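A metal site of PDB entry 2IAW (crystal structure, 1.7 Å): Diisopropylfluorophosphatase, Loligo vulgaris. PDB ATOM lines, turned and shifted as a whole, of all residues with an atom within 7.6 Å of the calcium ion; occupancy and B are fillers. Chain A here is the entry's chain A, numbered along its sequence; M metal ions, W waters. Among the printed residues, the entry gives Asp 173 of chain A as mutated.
Water W2 lies within hydrogen-bond range of the side-chain carboxylate (OD2) of Asp 119, the backbone NH (N) of Gly 228 and the side-chain amide oxygen (OD1) of Asn 270.
Water W3 lies within hydrogen-bond range of OD2 of Asp 173 (2.5 Å) and ND2 of Asn 118 (3.1 Å).
The side-chain hydroxyl (OG1) of Thr 131 is in hydrogen-bond range of the backbone carbonyl oxygen (O) of Asp 173 (2.6 Å).
The side-chain carboxylate of Asp 173 lies close to the side-chain hydroxyl of Thr 193.
OE1 of Glu 19 lies close to OD1 of Asn 270, at 2.9 Å.
The backbone carbonyl oxygen (O) of Asn 118 sits at hydrogen-bond distance from the backbone NH (N) of Gly 73, at 3.2 Å.
O of Thr 131 sits at hydrogen-bond distance from N of Asn 118 (2.9 Å).
ND2 of Asn 118 is in hydrogen-bond range of SD of Met 88 (3.6 Å).
The backbone NH of Gly 174 sits close to the backbone carbonyl oxygen of Asp 227, 3.0 Å away.
The calcium ion is bound by OD1 of Asp 173 (2.3 Å), OE2 of Glu 19 (2.4 Å), water W3 (2.4 Å), water W2 (2.4 Å), OD1 of Asn 118 (2.4 Å), water W1 (2.4 Å) and OD1 of Asp 227 (2.4 Å).
Four residues have an atom within 4 Å of the calcium ion: Glu 19, Asn 118, Asp 173 and Asp 227.
Along chain A the residues within 4 Å of the calcium ion span positions 19 to 227.
The nearest printed residue that does not touch the calcium ion is Asn 270 (4.4 Å).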
ATOM      1  N   GLU A  19      24.143  21.581 -19.361  1.00  0.00           N
ATOM      2  CA  GLU A  19      23.332  22.356 -18.406  1.00  0.00           C
ATOM      3  C   GLU A  19      22.891  23.661 -19.041  1.00  0.00           C
ATOM      4  O   GLU A  19      23.213  23.933 -20.193  1.00  0.00           O
ATOM      5  CB  GLU A  19      24.234  22.720 -17.210  1.00  0.00           C
ATOM      6  CG  GLU A  19      23.929  21.953 -15.920  1.00  0.00           C
ATOM      7  CD  GLU A  19      22.755  22.537 -15.133  1.00  0.00           C
ATOM      8  OE1 GLU A  19      21.929  23.246 -15.749  1.00  0.00           O
ATOM      9  OE2 GLU A  19      22.645  22.255 -13.913  1.00  0.00           O
ATOM     10  N   GLY A  20      22.132  24.474 -18.289  1.00  0.00           N
ATOM     11  CA  GLY A  20      21.769  25.821 -18.730  1.00  0.00           C
ATOM     12  C   GLY A  20      21.205  26.040 -20.114  1.00  0.00           C
ATOM     13  O   GLY A  20      21.617  26.996 -20.800  1.00  0.00           O
ATOM     14  N   ALA A  72      27.234  27.227 -15.571  1.00  0.00           N
ATOM     15  CA  ALA A  72      26.258  26.198 -15.194  1.00  0.00           C
ATOM     16  C   ALA A  72      24.795  26.506 -15.478  1.00  0.00           C
ATOM     17  O   ALA A  72      23.959  25.581 -15.550  1.00  0.00           O
ATOM     18  CB  ALA A  72      26.441  25.917 -13.689  1.00  0.00           C
ATOM     19  N   GLY A  73      24.451  27.773 -15.639  1.00  0.00           N
ATOM     20  CA  GLY A  73      23.051  28.098 -15.865  1.00  0.00           C
ATOM     21  C   GLY A  73      22.932  29.423 -16.559  1.00  0.00           C
ATOM     22  O   GLY A  73      23.787  30.294 -16.422  1.00  0.00           O
ATOM     23  N   MET A  88      30.102  28.455 -11.618  1.00  0.00           N
ATOM     24  CA  MET A  88      30.493  27.957 -10.300  1.00  0.00           C
ATOM     25  C   MET A  88      31.836  28.458  -9.782  1.00  0.00           C
ATOM     26  O   MET A  88      32.112  28.345  -8.600  1.00  0.00           O
ATOM     27  CB  MET A  88      30.442  26.433 -10.254  1.00  0.00           C
ATOM     28  CG  MET A  88      29.038  25.889 -10.357  1.00  0.00           C
ATOM     29  SD  MET A  88      28.006  25.973  -8.800  1.00  0.00           S
ATOM     30  CE  MET A  88      28.711  24.581  -7.878  1.00  0.00           C
ATOM     31  N   ASN A 118      25.072  28.820  -9.643  1.00  0.00           N
ATOM     32  CA  ASN A 118      24.644  27.659 -10.416  1.00  0.00           C
ATOM     33  C   ASN A 118      23.522  27.919 -11.428  1.00  0.00           C
ATOM     34  O   ASN A 118      23.589  27.476 -12.577  1.00  0.00           O
ATOM     35  CB  ASN A 118      24.199  26.575  -9.444  1.00  0.00           C
ATOM     36  CG  ASN A 118      24.019  25.234 -10.114  1.00  0.00           C
ATOM     37  OD1 ASN A 118      22.972  24.981 -10.720  1.00  0.00           O
ATOM     38  ND2 ASN A 118      25.082  24.381 -10.093  1.00  0.00           N
ATOM     39  N   ASP A 119      22.467  28.596 -10.984  1.00  0.00           N
ATOM     40  CA  ASP A 119      21.345  28.870 -11.909  1.00  0.00           C
ATOM     41  C   ASP A 119      20.735  30.221 -11.566  1.00  0.00           C
ATOM     42  O   ASP A 119      21.053  30.839 -10.529  1.00  0.00           O
ATOM     43  CB  ASP A 119      20.308  27.725 -11.848  1.00  0.00           C
ATOM     44  CG  ASP A 119      19.593  27.502 -13.188  1.00  0.00           C
ATOM     45  OD1 ASP A 119      19.755  28.327 -14.089  1.00  0.00           O
ATOM     46  OD2 ASP A 119      18.865  26.524 -13.402  1.00  0.00           O
ATOM     47  N   THR A 131      21.164  31.271  -7.602  1.00  0.00           N
ATOM     48  CA  THR A 131      21.594  30.358  -6.557  1.00  0.00           C
ATOM     49  C   THR A 131      23.102  30.282  -6.582  1.00  0.00           C
ATOM     50  O   THR A 131      23.741  30.389  -7.644  1.00  0.00           O
ATOM     51  CB  THR A 131      21.043  28.963  -6.756  1.00  0.00           C
ATOM     52  OG1 THR A 131      21.354  28.499  -8.097  1.00  0.00           O
ATOM     53  CG2 THR A 131      19.508  28.979  -6.649  1.00  0.00           C
ATOM     54  N   PRO A 133      25.583  27.728  -4.840  1.00  0.00           N
ATOM     55  CA  PRO A 133      25.954  26.597  -3.992  1.00  0.00           C
ATOM     56  C   PRO A 133      27.468  26.441  -3.832  1.00  0.00           C
ATOM     57  O   PRO A 133      27.888  25.644  -2.982  1.00  0.00           O
ATOM     58  CB  PRO A 133      25.348  25.382  -4.700  1.00  0.00           C
ATOM     59  CG  PRO A 133      25.452  25.799  -6.171  1.00  0.00           C
ATOM     60  CD  PRO A 133      25.218  27.326  -6.215  1.00  0.00           C
ATOM     61  N   PHE A 171      23.457  23.275  -0.986  1.00  0.00           N
ATOM     62  CA  PHE A 171      23.396  23.165  -2.436  1.00  0.00           C
ATOM     63  C   PHE A 171      22.102  23.683  -3.107  1.00  0.00           C
ATOM     64  O   PHE A 171      21.319  22.908  -3.693  1.00  0.00           O
ATOM     65  CB  PHE A 171      23.769  21.780  -2.945  1.00  0.00           C
ATOM     66  CG  PHE A 171      24.550  21.837  -4.235  1.00  0.00           C
ATOM     67  CD1 PHE A 171      23.896  22.001  -5.433  1.00  0.00           C
ATOM     68  CD2 PHE A 171      25.951  21.838  -4.223  1.00  0.00           C
ATOM     69  CE1 PHE A 171      24.620  22.115  -6.619  1.00  0.00           C
ATOM     70  CE2 PHE A 171      26.671  21.934  -5.378  1.00  0.00           C
ATOM     71  CZ  PHE A 171      26.024  22.086  -6.585  1.00  0.00           C
ATOM     72  N   PRO A 172      21.872  24.986  -3.038  1.00  0.00           N
ATOM     73  CA  PRO A 172      20.772  25.595  -3.759  1.00  0.00           C
ATOM     74  C   PRO A 172      21.111  25.476  -5.243  1.00  0.00           C
ATOM     75  O   PRO A 172      22.271  25.662  -5.633  1.00  0.00           O
ATOM     76  CB  PRO A 172      20.784  27.060  -3.256  1.00  0.00           C
ATOM     77  CG  PRO A 172      22.226  27.283  -2.947  1.00  0.00           C
ATOM     78  CD  PRO A 172      22.627  25.977  -2.266  1.00  0.00           C
ATOM     79  N   ASP A 173      20.114  25.176  -6.067  1.00  0.00           N
ATOM     80  CA  ASP A 173      20.414  24.801  -7.449  1.00  0.00           C
ATOM     81  C   ASP A 173      19.407  25.482  -8.387  1.00  0.00           C
ATOM     82  O   ASP A 173      19.605  26.612  -8.727  1.00  0.00           O
ATOM     83  CB  ASP A 173      20.390  23.280  -7.568  1.00  0.00           C
ATOM     84  CG  ASP A 173      21.102  22.780  -8.788  1.00  0.00           C
ATOM     85  OD1 ASP A 173      20.851  23.339  -9.880  1.00  0.00           O
ATOM     86  OD2 ASP A 173      21.967  21.881  -8.738  1.00  0.00           O
ATOM     87  N   GLY A 174      18.314  24.845  -8.746  1.00  0.00           N
ATOM     88  CA  GLY A 174      17.354  25.477  -9.635  1.00  0.00           C
ATOM     89  C   GLY A 174      16.654  26.631  -8.946  1.00  0.00           C
ATOM     90  O   GLY A 174      16.553  26.669  -7.703  1.00  0.00           O
ATOM     91  N   ILE A 175      16.100  27.536  -9.736  1.00  0.00           N
ATOM     92  CA  ILE A 175      15.397  28.655  -9.140  1.00  0.00           C
ATOM     93  C   ILE A 175      14.401  29.131 -10.177  1.00  0.00           C
ATOM     94  O   ILE A 175      14.623  28.997 -11.402  1.00  0.00           O
ATOM     95  CB  ILE A 175      16.439  29.745  -8.730  1.00  0.00           C
ATOM     96  CG1 ILE A 175      15.774  30.952  -8.033  1.00  0.00           C
ATOM     97  CG2 ILE A 175      17.346  30.127  -9.979  1.00  0.00           C
ATOM     98  CD1 ILE A 175      16.782  31.815  -7.268  1.00  0.00           C
ATOM     99  N   THR A 193      19.194  20.779  -3.508  1.00  0.00           N
ATOM    100  CA  THR A 193      19.257  19.454  -4.120  1.00  0.00           C
ATOM    101  C   THR A 193      19.216  18.238  -3.164  1.00  0.00           C
ATOM    102  O   THR A 193      18.305  17.405  -3.235  1.00  0.00           O
ATOM    103  CB  THR A 193      20.469  19.388  -5.077  1.00  0.00           C
ATOM    104  OG1 THR A 193      20.281  20.423  -6.060  1.00  0.00           O
ATOM    105  CG2 THR A 193      20.403  18.107  -5.879  1.00  0.00           C
ATOM    106  N   ALA A 226      16.322  17.818  -6.917  1.00  0.00           N
ATOM    107  CA  ALA A 226      15.923  18.875  -7.857  1.00  0.00           C
ATOM    108  C   ALA A 226      17.142  19.594  -8.375  1.00  0.00           C
ATOM    109  O   ALA A 226      17.988  20.046  -7.605  1.00  0.00           O
ATOM    110  CB  ALA A 226      14.981  19.909  -7.168  1.00  0.00           C
ATOM    111  N   ASP A 227      17.170  19.781  -9.679  1.00  0.00           N
ATOM    112  CA  ASP A 227      18.255  20.496 -10.326  1.00  0.00           C
ATOM    113  C   ASP A 227      17.575  21.698 -10.994  1.00  0.00           C
ATOM    114  O   ASP A 227      17.105  22.569 -10.280  1.00  0.00           O
ATOM    115  CB  ASP A 227      18.933  19.550 -11.301  1.00  0.00           C
ATOM    116  CG  ASP A 227      20.291  20.033 -11.788  1.00  0.00           C
ATOM    117  OD1 ASP A 227      20.503  21.266 -11.808  1.00  0.00           O
ATOM    118  OD2 ASP A 227      21.177  19.211 -12.187  1.00  0.00           O
ATOM    119  N   GLY A 228      17.425  21.753 -12.330  1.00  0.00           N
ATOM    120  CA  GLY A 228      16.788  22.940 -12.934  1.00  0.00           C
ATOM    121  C   GLY A 228      15.259  22.897 -12.955  1.00  0.00           C
ATOM    122  O   GLY A 228      14.643  21.846 -12.850  1.00  0.00           O
ATOM    123  N   MET A 229      14.641  24.061 -13.111  1.00  0.00           N
ATOM    124  CA  MET A 229      13.177  24.154 -13.138  1.00  0.00           C
ATOM    125  C   MET A 229      12.705  25.297 -14.004  1.00  0.00           C
ATOM    126  O   MET A 229      13.468  26.222 -14.286  1.00  0.00           O
ATOM    127  CB  MET A 229      12.645  24.428 -11.711  1.00  0.00           C
ATOM    128  CG  MET A 229      13.208  25.705 -11.120  1.00  0.00           C
ATOM    129  SD  MET A 229      12.601  26.048  -9.439  1.00  0.00           S
ATOM    130  CE  MET A 229      13.244  24.567  -8.721  1.00  0.00           C
ATOM    131  N   SER A 269      19.118  17.232 -15.982  1.00  0.00           N
ATOM    132  CA  SER A 269      19.786  18.268 -15.188  1.00  0.00           C
ATOM    133  C   SER A 269      19.053  19.587 -15.287  1.00  0.00           C
ATOM    134  O   SER A 269      19.001  20.340 -14.321  1.00  0.00           O
ATOM    135  CB  SER A 269      21.234  18.468 -15.672  1.00  0.00           C
ATOM    136  OG  SER A 269      21.230  18.933 -17.014  1.00  0.00           O
ATOM    137  N   ASN A 270      18.526  19.914 -16.470  1.00  0.00           N
ATOM    138  CA  ASN A 270      17.892  21.217 -16.589  1.00  0.00           C
ATOM    139  C   ASN A 270      16.976  21.238 -17.793  1.00  0.00           C
ATOM    140  O   ASN A 270      16.960  20.289 -18.569  1.00  0.00           O
ATOM    141  CB  ASN A 270      18.966  22.337 -16.653  1.00  0.00           C
ATOM    142  CG  ASN A 270      18.515  23.652 -16.013  1.00  0.00           C
ATOM    143  OD1 ASN A 270      19.350  24.428 -15.465  1.00  0.00           O
ATOM    144  ND2 ASN A 270      17.226  23.938 -16.060  1.00  0.00           N
ATOM    145  N   HIS A 285      22.796  14.166 -17.816  1.00  0.00           N
ATOM    146  CA  HIS A 285      24.172  13.749 -17.547  1.00  0.00           C
ATOM    147  C   HIS A 285      24.463  12.273 -17.603  1.00  0.00           C
ATOM    148  O   HIS A 285      25.584  11.846 -17.302  1.00  0.00           O
ATOM    149  CB  HIS A 285      24.590  14.293 -16.175  1.00  0.00           C
ATOM    150  CG  HIS A 285      24.537  15.777 -16.065  1.00  0.00           C
ATOM    151  ND1 HIS A 285      24.511  16.427 -14.855  1.00  0.00           N
ATOM    152  CD2 HIS A 285      24.508  16.749 -17.012  1.00  0.00           C
ATOM    153  CE1 HIS A 285      24.469  17.739 -15.047  1.00  0.00           C
ATOM    154  NE2 HIS A 285      24.465  17.951 -16.357  1.00  0.00           N
HETATM  155 CA    CA M   1      21.800  23.322 -11.995  1.00  0.00          CA
HETATM  156  O   HOH W   1      22.127  25.182 -13.505  1.00  0.00           O
HETATM  157  O   HOH W   2      19.634  24.319 -11.997  1.00  0.00           O
HETATM  158  O   HOH W   3      23.348  21.943 -10.864  1.00  0.00           O
